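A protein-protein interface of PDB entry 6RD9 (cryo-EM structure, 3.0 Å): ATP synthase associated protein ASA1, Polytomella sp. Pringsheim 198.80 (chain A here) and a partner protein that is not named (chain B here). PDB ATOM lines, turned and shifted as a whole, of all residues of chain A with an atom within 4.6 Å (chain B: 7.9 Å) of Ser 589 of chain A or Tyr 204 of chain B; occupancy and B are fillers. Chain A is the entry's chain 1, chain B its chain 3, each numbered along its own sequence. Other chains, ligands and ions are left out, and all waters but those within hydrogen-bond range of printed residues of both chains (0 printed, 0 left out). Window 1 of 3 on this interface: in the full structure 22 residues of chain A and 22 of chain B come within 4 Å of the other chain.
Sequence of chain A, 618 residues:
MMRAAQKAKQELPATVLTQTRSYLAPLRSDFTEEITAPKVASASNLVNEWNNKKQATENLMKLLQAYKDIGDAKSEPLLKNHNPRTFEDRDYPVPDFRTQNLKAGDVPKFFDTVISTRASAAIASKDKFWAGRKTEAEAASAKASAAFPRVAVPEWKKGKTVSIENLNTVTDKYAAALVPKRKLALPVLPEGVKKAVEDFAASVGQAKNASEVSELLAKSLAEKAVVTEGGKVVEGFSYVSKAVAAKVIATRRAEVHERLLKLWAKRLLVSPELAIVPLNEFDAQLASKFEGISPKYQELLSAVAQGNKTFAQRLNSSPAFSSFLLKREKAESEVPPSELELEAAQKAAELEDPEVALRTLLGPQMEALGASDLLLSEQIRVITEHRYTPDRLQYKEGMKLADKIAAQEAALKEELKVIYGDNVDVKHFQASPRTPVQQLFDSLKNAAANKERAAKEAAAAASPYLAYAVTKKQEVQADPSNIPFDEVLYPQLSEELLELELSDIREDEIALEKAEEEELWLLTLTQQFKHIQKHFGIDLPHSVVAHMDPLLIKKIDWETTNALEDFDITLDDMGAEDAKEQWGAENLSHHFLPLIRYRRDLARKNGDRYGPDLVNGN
NZ of Lys 555 of chain A is in hydrogen-bond range of O of Tyr 204 of chain B (2.7 Å).
OD2 of Asp 235 of chain B is in hydrogen-bond range of OH of Tyr 204 of chain B (2.8 Å). NZ of Lys 555 of chain A is in hydrogen-bond range of O of Glu 586 of chain A, at 3.4 Å. The guanidinium group (NH1) of Arg 233 of chain B lies within salt-bridge range of the side-chain carboxylate (OD1) of Asp 200 of chain B, 2.9 Å away. A ring nitrogen (NE2) of His 590 of chain A sits at hydrogen-bond distance from the backbone carbonyl oxygen (O) of Asn 587 of chain A (3.1 Å). The backbone NH (N) of Cys 205 of chain B lies within hydrogen-bond range of the backbone carbonyl oxygen (O) of Asp 200 of chain B (3.5 Å). The backbone carbonyl oxygen (O) of Phe 169 of chain B sits at hydrogen-bond distance from the side-chain hydroxyl (OG) of Ser 201 of chain B (2.8 Å).
CD2 of His 207 of chain B touches O of Lys 555 of chain A (3.2 Å). OE1 of Glu 586 of chain A touches CB of Tyr 208 of chain B, 3.5 Å away. His 207 of chain B touches Asn 587 of chain A (CD2 to ND2, 3.7 Å). CD1 of Tyr 204 of chain B touches OG of Ser 589 of chain A, at 3.3 Å. His 590 of chain A touches Tyr 204 of chain B. CE2 of Phe 169 of chain B touches CD2 of Leu 593 of chain A, 3.998 Å away. CD1 of Leu 593 of chain A touches CG of Asp 200 of chain B, at 3.9 Å. CD1 of Leu 593 of chain A touches CD2 of Tyr 204 of chain B, at 3.7 Å. Cys 205 of chain B touches Leu 593 of chain A (SG to CD2, 3.7 Å). Tyr 204 of chain B touches Ile 596 of chain A.
Printed residues of chain B within 4 Å of Ser 589 of chain A: Tyr 204. Tyr 204 of chain B touches five residues of chain A. Of the printed residues of chain A, Cys 205 of chain B touches Leu 593 (3.7 Å). Of the printed residues of chain B, His 590 of chain A touches Tyr 204 (3.4 Å). Printed residues of chain B within 4 Å of Asn 587 of chain A: His 207. Printed residues of chain A within 4 Å of Tyr 208 of chain B: Glu 586. Printed residues of chain B within 4 Å of Ile 596 of chain A: Tyr 204. Thr 170 of chain B touches none of the printed residues of chain A. Thr 203 of chain B touches none of the printed residues of chain A. The nearest residue of chain B that does not touch Ser 589 of chain A is Thr 203 of chain B (4.3 Å). The nearest printed residue of chain A that does not touch Tyr 204 of chain B is Glu 586 of chain A (5.4 Å).
Hydrophobic or aromatic side chains of chain B within 4 Å of the printed part of chain A: Phe 169, Tyr 204, His 207 and Tyr 208. Of the 11 printed residues of chain A, 7 touch a printed residue of chain B. Printed residues of chain A that touch a printed residue of chain B: Lys 555, Glu 586, Asn 587, Ser 589, His 590, Leu 593 and Ile 596. Hydrophobic or aromatic side chains of chain A within 4 Å of the printed part of chain B: His 590, Leu 593 and Ile 596.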
ATOM      1  N   LYS A 555      -2.594 -23.872 -19.138  1.00  0.00           N
ATOM      2  CA  LYS A 555      -1.896 -25.100 -19.477  1.00  0.00           C
ATOM      3  C   LYS A 555      -2.715 -26.004 -20.372  1.00  0.00           C
ATOM      4  O   LYS A 555      -2.144 -26.805 -21.099  1.00  0.00           O
ATOM      5  CB  LYS A 555      -1.544 -25.863 -18.220  1.00  0.00           C
ATOM      6  CG  LYS A 555      -0.572 -25.198 -17.353  1.00  0.00           C
ATOM      7  CD  LYS A 555      -0.285 -26.050 -16.193  1.00  0.00           C
ATOM      8  CE  LYS A 555      -0.156 -25.250 -14.983  1.00  0.00           C
ATOM      9  NZ  LYS A 555       0.561 -26.008 -13.979  1.00  0.00           N
ATOM     10  N   ALA A 585      -1.515 -34.442 -12.388  1.00  0.00           N
ATOM     11  CA  ALA A 585      -0.920 -33.814 -11.225  1.00  0.00           C
ATOM     12  C   ALA A 585      -0.064 -32.625 -11.590  1.00  0.00           C
ATOM     13  O   ALA A 585       0.045 -31.693 -10.801  1.00  0.00           O
ATOM     14  CB  ALA A 585      -0.079 -34.816 -10.461  1.00  0.00           C
ATOM     15  N   GLU A 586       0.548 -32.629 -12.758  1.00  0.00           N
ATOM     16  CA  GLU A 586       1.354 -31.503 -13.188  1.00  0.00           C
ATOM     17  C   GLU A 586       0.533 -30.370 -13.756  1.00  0.00           C
ATOM     18  O   GLU A 586       1.092 -29.316 -14.045  1.00  0.00           O
ATOM     19  CB  GLU A 586       2.359 -31.936 -14.233  1.00  0.00           C
ATOM     20  CG  GLU A 586       3.479 -32.756 -13.698  1.00  0.00           C
ATOM     21  CD  GLU A 586       4.571 -31.945 -13.083  1.00  0.00           C
ATOM     22  OE1 GLU A 586       4.699 -30.760 -13.426  1.00  0.00           O
ATOM     23  OE2 GLU A 586       5.311 -32.497 -12.249  1.00  0.00           O
ATOM     24  N   ASN A 587      -0.756 -30.563 -13.971  1.00  0.00           N
ATOM     25  CA  ASN A 587      -1.605 -29.510 -14.485  1.00  0.00           C
ATOM     26  C   ASN A 587      -2.376 -28.815 -13.401  1.00  0.00           C
ATOM     27  O   ASN A 587      -2.892 -27.723 -13.631  1.00  0.00           O
ATOM     28  CB  ASN A 587      -2.595 -30.059 -15.498  1.00  0.00           C
ATOM     29  CG  ASN A 587      -2.018 -30.166 -16.869  1.00  0.00           C
ATOM     30  OD1 ASN A 587      -2.634 -30.702 -17.764  1.00  0.00           O
ATOM     31  ND2 ASN A 587      -0.823 -29.656 -17.044  1.00  0.00           N
ATOM     32  N   LEU A 588      -2.495 -29.440 -12.246  1.00  0.00           N
ATOM     33  CA  LEU A 588      -2.937 -28.793 -11.032  1.00  0.00           C
ATOM     34  C   LEU A 588      -1.777 -28.515 -10.117  1.00  0.00           C
ATOM     35  O   LEU A 588      -1.966 -28.357  -8.919  1.00  0.00           O
ATOM     36  CB  LEU A 588      -3.962 -29.669 -10.342  1.00  0.00           C
ATOM     37  CG  LEU A 588      -5.072 -30.062 -11.277  1.00  0.00           C
ATOM     38  CD1 LEU A 588      -5.776 -31.149 -10.645  1.00  0.00           C
ATOM     39  CD2 LEU A 588      -5.960 -28.907 -11.437  1.00  0.00           C
ATOM     40  N   SER A 589      -0.578 -28.462 -10.672  1.00  0.00           N
ATOM     41  CA  SER A 589       0.651 -28.332  -9.919  1.00  0.00           C
ATOM     42  C   SER A 589       0.780 -26.983  -9.269  1.00  0.00           C
ATOM     43  O   SER A 589       1.484 -26.851  -8.273  1.00  0.00           O
ATOM     44  CB  SER A 589       1.816 -28.541 -10.863  1.00  0.00           C
ATOM     45  OG  SER A 589       3.036 -28.424 -10.191  1.00  0.00           O
ATOM     46  N   HIS A 590       0.127 -25.996  -9.825  1.00  0.00           N
ATOM     47  CA  HIS A 590       0.140 -24.626  -9.392  1.00  0.00           C
ATOM     48  C   HIS A 590      -0.813 -24.366  -8.257  1.00  0.00           C
ATOM     49  O   HIS A 590      -0.934 -23.226  -7.829  1.00  0.00           O
ATOM     50  CB  HIS A 590      -0.241 -23.741 -10.555  1.00  0.00           C
ATOM     51  CG  HIS A 590      -1.566 -24.092 -11.141  1.00  0.00           C
ATOM     52  ND1 HIS A 590      -2.719 -23.437 -10.796  1.00  0.00           N
ATOM     53  CD2 HIS A 590      -1.930 -25.052 -12.015  1.00  0.00           C
ATOM     54  CE1 HIS A 590      -3.733 -23.972 -11.438  1.00  0.00           C
ATOM     55  NE2 HIS A 590      -3.279 -24.950 -12.188  1.00  0.00           N
ATOM     56  N   HIS A 591      -1.546 -25.370  -7.803  1.00  0.00           N
ATOM     57  CA  HIS A 591      -2.421 -25.165  -6.665  1.00  0.00           C
ATOM     58  C   HIS A 591      -1.627 -25.096  -5.387  1.00  0.00           C
ATOM     59  O   HIS A 591      -2.072 -24.493  -4.415  1.00  0.00           O
ATOM     60  CB  HIS A 591      -3.446 -26.277  -6.584  1.00  0.00           C
ATOM     61  CG  HIS A 591      -4.585 -26.112  -7.528  1.00  0.00           C
ATOM     62  ND1 HIS A 591      -5.684 -26.928  -7.518  1.00  0.00           N
ATOM     63  CD2 HIS A 591      -4.806 -25.201  -8.493  1.00  0.00           C
ATOM     64  CE1 HIS A 591      -6.526 -26.540  -8.451  1.00  0.00           C
ATOM     65  NE2 HIS A 591      -6.016 -25.492  -9.057  1.00  0.00           N
ATOM     66  N   PHE A 592      -0.457 -25.698  -5.381  1.00  0.00           N
ATOM     67  CA  PHE A 592       0.447 -25.722  -4.255  1.00  0.00           C
ATOM     68  C   PHE A 592       1.486 -24.635  -4.338  1.00  0.00           C
ATOM     69  O   PHE A 592       2.297 -24.514  -3.432  1.00  0.00           O
ATOM     70  CB  PHE A 592       1.123 -27.075  -4.187  1.00  0.00           C
ATOM     71  CG  PHE A 592       0.172 -28.203  -4.134  1.00  0.00           C
ATOM     72  CD1 PHE A 592      -0.383 -28.581  -2.944  1.00  0.00           C
ATOM     73  CD2 PHE A 592      -0.182 -28.881  -5.264  1.00  0.00           C
ATOM     74  CE1 PHE A 592      -1.267 -29.597  -2.887  1.00  0.00           C
ATOM     75  CE2 PHE A 592      -1.074 -29.901  -5.195  1.00  0.00           C
ATOM     76  CZ  PHE A 592      -1.604 -30.258  -3.999  1.00  0.00           C
ATOM     77  N   LEU A 593       1.482 -23.866  -5.409  1.00  0.00           N
ATOM     78  CA  LEU A 593       2.401 -22.743  -5.536  1.00  0.00           C
ATOM     79  C   LEU A 593       2.159 -21.599  -4.553  1.00  0.00           C
ATOM     80  O   LEU A 593       3.158 -21.016  -4.103  1.00  0.00           O
ATOM     81  CB  LEU A 593       2.380 -22.226  -6.972  1.00  0.00           C
ATOM     82  CG  LEU A 593       3.342 -21.106  -7.308  1.00  0.00           C
ATOM     83  CD1 LEU A 593       4.719 -21.588  -7.057  1.00  0.00           C
ATOM     84  CD2 LEU A 593       3.181 -20.703  -8.707  1.00  0.00           C
ATOM     85  N   ILE A 596       4.067 -22.990  -1.392  1.00  0.00           N
ATOM     86  CA  ILE A 596       5.513 -23.123  -1.405  1.00  0.00           C
ATOM     87  C   ILE A 596       6.213 -21.859  -1.843  1.00  0.00           C
ATOM     88  O   ILE A 596       7.437 -21.820  -1.841  1.00  0.00           O
ATOM     89  CB  ILE A 596       5.933 -24.315  -2.275  1.00  0.00           C
ATOM     90  CG1 ILE A 596       5.778 -24.000  -3.741  1.00  0.00           C
ATOM     91  CG2 ILE A 596       5.108 -25.524  -1.897  1.00  0.00           C
ATOM     92  CD1 ILE A 596       5.922 -25.187  -4.591  1.00  0.00           C
ATOM     93  N   PHE B 169       4.848 -13.254 -13.194  1.00  0.00           N
ATOM     94  CA  PHE B 169       5.514 -14.494 -13.552  1.00  0.00           C
ATOM     95  C   PHE B 169       4.541 -15.584 -13.946  1.00  0.00           C
ATOM     96  O   PHE B 169       4.931 -16.514 -14.646  1.00  0.00           O
ATOM     97  CB  PHE B 169       6.419 -14.952 -12.413  1.00  0.00           C
ATOM     98  CG  PHE B 169       5.698 -15.523 -11.236  1.00  0.00           C
ATOM     99  CD1 PHE B 169       5.067 -14.707 -10.330  1.00  0.00           C
ATOM    100  CD2 PHE B 169       5.695 -16.875 -11.011  1.00  0.00           C
ATOM    101  CE1 PHE B 169       4.419 -15.235  -9.262  1.00  0.00           C
ATOM    102  CE2 PHE B 169       5.051 -17.395  -9.951  1.00  0.00           C
ATOM    103  CZ  PHE B 169       4.416 -16.577  -9.075  1.00  0.00           C
ATOM    104  N   THR B 170       3.280 -15.479 -13.555  1.00  0.00           N
ATOM    105  CA  THR B 170       2.328 -16.498 -13.941  1.00  0.00           C
ATOM    106  C   THR B 170       1.914 -16.373 -15.393  1.00  0.00           C
ATOM    107  O   THR B 170       1.388 -17.334 -15.952  1.00  0.00           O
ATOM    108  CB  THR B 170       1.104 -16.429 -13.053  1.00  0.00           C
ATOM    109  OG1 THR B 170       0.451 -15.187 -13.264  1.00  0.00           O
ATOM    110  CG2 THR B 170       1.500 -16.497 -11.645  1.00  0.00           C
ATOM    111  N   ASP B 196      13.870 -17.087  -8.660  1.00  0.00           N
ATOM    112  CA  ASP B 196      12.786 -17.898  -8.140  1.00  0.00           C
ATOM    113  C   ASP B 196      11.534 -17.763  -8.982  1.00  0.00           C
ATOM    114  O   ASP B 196      10.868 -18.759  -9.245  1.00  0.00           O
ATOM    115  CB  ASP B 196      12.489 -17.507  -6.700  1.00  0.00           C
ATOM    116  CG  ASP B 196      13.345 -18.254  -5.713  1.00  0.00           C
ATOM    117  OD1 ASP B 196      13.685 -19.416  -5.979  1.00  0.00           O
ATOM    118  OD2 ASP B 196      13.664 -17.688  -4.657  1.00  0.00           O
ATOM    119  N   VAL B 198      11.341 -17.060 -12.142  1.00  0.00           N
ATOM    120  CA  VAL B 198      11.474 -17.749 -13.415  1.00  0.00           C
ATOM    121  C   VAL B 198      11.365 -19.248 -13.204  1.00  0.00           C
ATOM    122  O   VAL B 198      10.736 -19.956 -13.989  1.00  0.00           O
ATOM    123  CB  VAL B 198      12.782 -17.326 -14.102  1.00  0.00           C
ATOM    124  CG1 VAL B 198      13.263 -18.346 -15.071  1.00  0.00           C
ATOM    125  CG2 VAL B 198      12.542 -16.068 -14.848  1.00  0.00           C
ATOM    126  N   ALA B 199      11.915 -19.748 -12.110  1.00  0.00           N
ATOM    127  CA  ALA B 199      11.812 -21.169 -11.823  1.00  0.00           C
ATOM    128  C   ALA B 199      10.433 -21.553 -11.328  1.00  0.00           C
ATOM    129  O   ALA B 199      10.018 -22.697 -11.507  1.00  0.00           O
ATOM    130  CB  ALA B 199      12.852 -21.565 -10.793  1.00  0.00           C
ATOM    131  N   ASP B 200       9.722 -20.637 -10.670  1.00  0.00           N
ATOM    132  CA  ASP B 200       8.357 -20.927 -10.254  1.00  0.00           C
ATOM    133  C   ASP B 200       7.427 -20.954 -11.439  1.00  0.00           C
ATOM    134  O   ASP B 200       6.421 -21.657 -11.420  1.00  0.00           O
ATOM    135  CB  ASP B 200       7.856 -19.891  -9.262  1.00  0.00           C
ATOM    136  CG  ASP B 200       8.308 -20.160  -7.856  1.00  0.00           C
ATOM    137  OD1 ASP B 200       8.843 -21.248  -7.598  1.00  0.00           O
ATOM    138  OD2 ASP B 200       8.127 -19.278  -6.996  1.00  0.00           O
ATOM    139  N   SER B 201       7.750 -20.199 -12.470  1.00  0.00           N
ATOM    140  CA  SER B 201       6.892 -20.073 -13.624  1.00  0.00           C
ATOM    141  C   SER B 201       7.102 -21.196 -14.615  1.00  0.00           C
ATOM    142  O   SER B 201       6.154 -21.644 -15.244  1.00  0.00           O
ATOM    143  CB  SER B 201       7.158 -18.746 -14.292  1.00  0.00           C
ATOM    144  OG  SER B 201       6.447 -18.673 -15.493  1.00  0.00           O
ATOM    145  N   ILE B 202       8.333 -21.654 -14.781  1.00  0.00           N
ATOM    146  CA  ILE B 202       8.595 -22.767 -15.674  1.00  0.00           C
ATOM    147  C   ILE B 202       8.063 -24.054 -15.083  1.00  0.00           C
ATOM    148  O   ILE B 202       7.568 -24.924 -15.804  1.00  0.00           O
ATOM    149  CB  ILE B 202      10.102 -22.815 -15.980  1.00  0.00           C
ATOM    150  CG1 ILE B 202      10.460 -21.684 -16.923  1.00  0.00           C
ATOM    151  CG2 ILE B 202      10.530 -24.099 -16.612  1.00  0.00           C
ATOM    152  CD1 ILE B 202      11.896 -21.578 -17.224  1.00  0.00           C
ATOM    153  N   THR B 203       8.074 -24.174 -13.764  1.00  0.00           N
ATOM    154  CA  THR B 203       7.717 -25.436 -13.138  1.00  0.00           C
ATOM    155  C   THR B 203       6.228 -25.538 -12.872  1.00  0.00           C
ATOM    156  O   THR B 203       5.618 -26.579 -13.120  1.00  0.00           O
ATOM    157  CB  THR B 203       8.474 -25.592 -11.844  1.00  0.00           C
ATOM    158  OG1 THR B 203       9.814 -25.188 -12.051  1.00  0.00           O
ATOM    159  CG2 THR B 203       8.472 -27.009 -11.445  1.00  0.00           C
ATOM    160  N   TYR B 204       5.630 -24.477 -12.348  1.00  0.00           N
ATOM    161  CA  TYR B 204       4.265 -24.514 -11.859  1.00  0.00           C
ATOM    162  C   TYR B 204       3.291 -23.750 -12.718  1.00  0.00           C
ATOM    163  O   TYR B 204       2.160 -24.180 -12.863  1.00  0.00           O
ATOM    164  CB  TYR B 204       4.201 -23.960 -10.437  1.00  0.00           C
ATOM    165  CG  TYR B 204       5.104 -24.684  -9.509  1.00  0.00           C
ATOM    166  CD1 TYR B 204       4.748 -25.900  -9.006  1.00  0.00           C
ATOM    167  CD2 TYR B 204       6.321 -24.158  -9.150  1.00  0.00           C
ATOM    168  CE1 TYR B 204       5.571 -26.577  -8.187  1.00  0.00           C
ATOM    169  CE2 TYR B 204       7.154 -24.830  -8.330  1.00  0.00           C
ATOM    170  CZ  TYR B 204       6.776 -26.040  -7.855  1.00  0.00           C
ATOM    171  OH  TYR B 204       7.603 -26.727  -7.018  1.00  0.00           O
ATOM    172  N   CYS B 205       3.686 -22.635 -13.285  1.00  0.00           N
ATOM    173  CA  CYS B 205       2.757 -21.841 -14.055  1.00  0.00           C
ATOM    174  C   CYS B 205       2.728 -22.228 -15.517  1.00  0.00           C
ATOM    175  O   CYS B 205       1.984 -21.620 -16.281  1.00  0.00           O
ATOM    176  CB  CYS B 205       3.110 -20.369 -13.924  1.00  0.00           C
ATOM    177  SG  CYS B 205       3.212 -19.770 -12.255  1.00  0.00           S
ATOM    178  N   ASN B 206       3.519 -23.202 -15.931  1.00  0.00           N
ATOM    179  CA  ASN B 206       3.603 -23.584 -17.323  1.00  0.00           C
ATOM    180  C   ASN B 206       3.456 -25.077 -17.459  1.00  0.00           C
ATOM    181  O   ASN B 206       3.709 -25.823 -16.518  1.00  0.00           O
ATOM    182  CB  ASN B 206       4.907 -23.147 -17.930  1.00  0.00           C
ATOM    183  CG  ASN B 206       4.836 -21.783 -18.468  1.00  0.00           C
ATOM    184  OD1 ASN B 206       5.398 -20.854 -17.930  1.00  0.00           O
ATOM    185  ND2 ASN B 206       4.145 -21.647 -19.565  1.00  0.00           N
ATOM    186  N   HIS B 207       3.051 -25.499 -18.656  1.00  0.00           N
ATOM    187  CA  HIS B 207       2.803 -26.902 -18.931  1.00  0.00           C
ATOM    188  C   HIS B 207       4.073 -27.706 -18.765  1.00  0.00           C
ATOM    189  O   HIS B 207       5.162 -27.230 -19.057  1.00  0.00           O
ATOM    190  CB  HIS B 207       2.273 -27.079 -20.337  1.00  0.00           C
ATOM    191  CG  HIS B 207       1.591 -28.385 -20.553  1.00  0.00           C
ATOM    192  ND1 HIS B 207       2.270 -29.529 -20.878  1.00  0.00           N
ATOM    193  CD2 HIS B 207       0.296 -28.738 -20.455  1.00  0.00           C
ATOM    194  CE1 HIS B 207       1.424 -30.529 -20.986  1.00  0.00           C
ATOM    195  NE2 HIS B 207       0.218 -30.075 -20.727  1.00  0.00           N
ATOM    196  N   TYR B 208       3.942 -28.919 -18.254  1.00  0.00           N
ATOM    197  CA  TYR B 208       5.131 -29.660 -17.888  1.00  0.00           C
ATOM    198  C   TYR B 208       5.854 -30.243 -19.081  1.00  0.00           C
ATOM    199  O   TYR B 208       6.988 -30.691 -18.930  1.00  0.00           O
ATOM    200  CB  TYR B 208       4.766 -30.739 -16.883  1.00  0.00           C
ATOM    201  CG  TYR B 208       4.153 -32.000 -17.394  1.00  0.00           C
ATOM    202  CD1 TYR B 208       2.896 -32.015 -17.939  1.00  0.00           C
ATOM    203  CD2 TYR B 208       4.810 -33.187 -17.256  1.00  0.00           C
ATOM    204  CE1 TYR B 208       2.349 -33.179 -18.385  1.00  0.00           C
ATOM    205  CE2 TYR B 208       4.270 -34.337 -17.684  1.00  0.00           C
ATOM    206  CZ  TYR B 208       3.048 -34.330 -18.249  1.00  0.00           C
ATOM    207  OH  TYR B 208       2.539 -35.513 -18.663  1.00  0.00           O
ATOM    208  N   ARG B 233      17.320 -25.110  -7.407  1.00  0.00           N
ATOM    209  CA  ARG B 233      15.875 -25.309  -7.427  1.00  0.00           C
ATOM    210  C   ARG B 233      15.704 -26.711  -7.969  1.00  0.00           C
ATOM    211  O   ARG B 233      15.721 -26.885  -9.179  1.00  0.00           O
ATOM    212  CB  ARG B 233      15.188 -24.295  -8.309  1.00  0.00           C
ATOM    213  CG  ARG B 233      15.189 -22.892  -7.798  1.00  0.00           C
ATOM    214  CD  ARG B 233      14.213 -22.751  -6.684  1.00  0.00           C
ATOM    215  NE  ARG B 233      12.967 -23.408  -7.011  1.00  0.00           N
ATOM    216  CZ  ARG B 233      11.885 -22.773  -7.416  1.00  0.00           C
ATOM    217  NH1 ARG B 233      10.790 -23.447  -7.693  1.00  0.00           N
ATOM    218  NH2 ARG B 233      11.903 -21.464  -7.528  1.00  0.00           N
ATOM    219  N   ALA B 234      15.551 -27.705  -7.101  1.00  0.00           N
ATOM    220  CA  ALA B 234      15.506 -29.080  -7.578  1.00  0.00           C
ATOM    221  C   ALA B 234      14.212 -29.410  -8.287  1.00  0.00           C
ATOM    222  O   ALA B 234      14.131 -30.448  -8.945  1.00  0.00           O
ATOM    223  CB  ALA B 234      15.698 -30.056  -6.431  1.00  0.00           C
ATOM    224  N   ASP B 235      13.189 -28.578  -8.132  1.00  0.00           N
ATOM    225  CA  ASP B 235      11.958 -28.765  -8.880  1.00  0.00           C
ATOM    226  C   ASP B 235      12.098 -28.270 -10.308  1.00  0.00           C
ATOM    227  O   ASP B 235      11.543 -28.873 -11.229  1.00  0.00           O
ATOM    228  CB  ASP B 235      10.813 -28.079  -8.148  1.00  0.00           C
ATOM    229  CG  ASP B 235      11.119 -26.652  -7.778  1.00  0.00           C
ATOM    230  OD1 ASP B 235      12.202 -26.159  -8.091  1.00  0.00           O
ATOM    231  OD2 ASP B 235      10.285 -26.014  -7.125  1.00  0.00           O
ATOM    232  N   LEU B 236      12.846 -27.185 -10.512  1.00  0.00           N
ATOM    233  CA  LEU B 236      13.106 -26.695 -11.856  1.00  0.00           C
ATOM    234  C   LEU B 236      13.997 -27.648 -12.622  1.00  0.00           C
ATOM    235  O   LEU B 236      13.836 -27.817 -13.827  1.00  0.00           O
ATOM    236  CB  LEU B 236      13.749 -25.317 -11.796  1.00  0.00           C
ATOM    237  CG  LEU B 236      14.199 -24.693 -13.109  1.00  0.00           C
ATOM    238  CD1 LEU B 236      13.042 -24.133 -13.830  1.00  0.00           C
ATOM    239  CD2 LEU B 236      15.201 -23.629 -12.876  1.00  0.00           C
ATOM    240  N   THR B 239      12.160 -30.412 -14.240  1.00  0.00           N
ATOM    241  CA  THR B 239      11.365 -29.920 -15.349  1.00  0.00           C
ATOM    242  C   THR B 239      12.210 -29.742 -16.596  1.00  0.00           C
ATOM    243  O   THR B 239      11.836 -30.215 -17.666  1.00  0.00           O
ATOM    244  CB  THR B 239      10.708 -28.605 -14.941  1.00  0.00           C
ATOM    245  OG1 THR B 239       9.806 -28.852 -13.870  1.00  0.00           O
ATOM    246  CG2 THR B 239       9.942 -28.025 -16.036  1.00  0.00           C
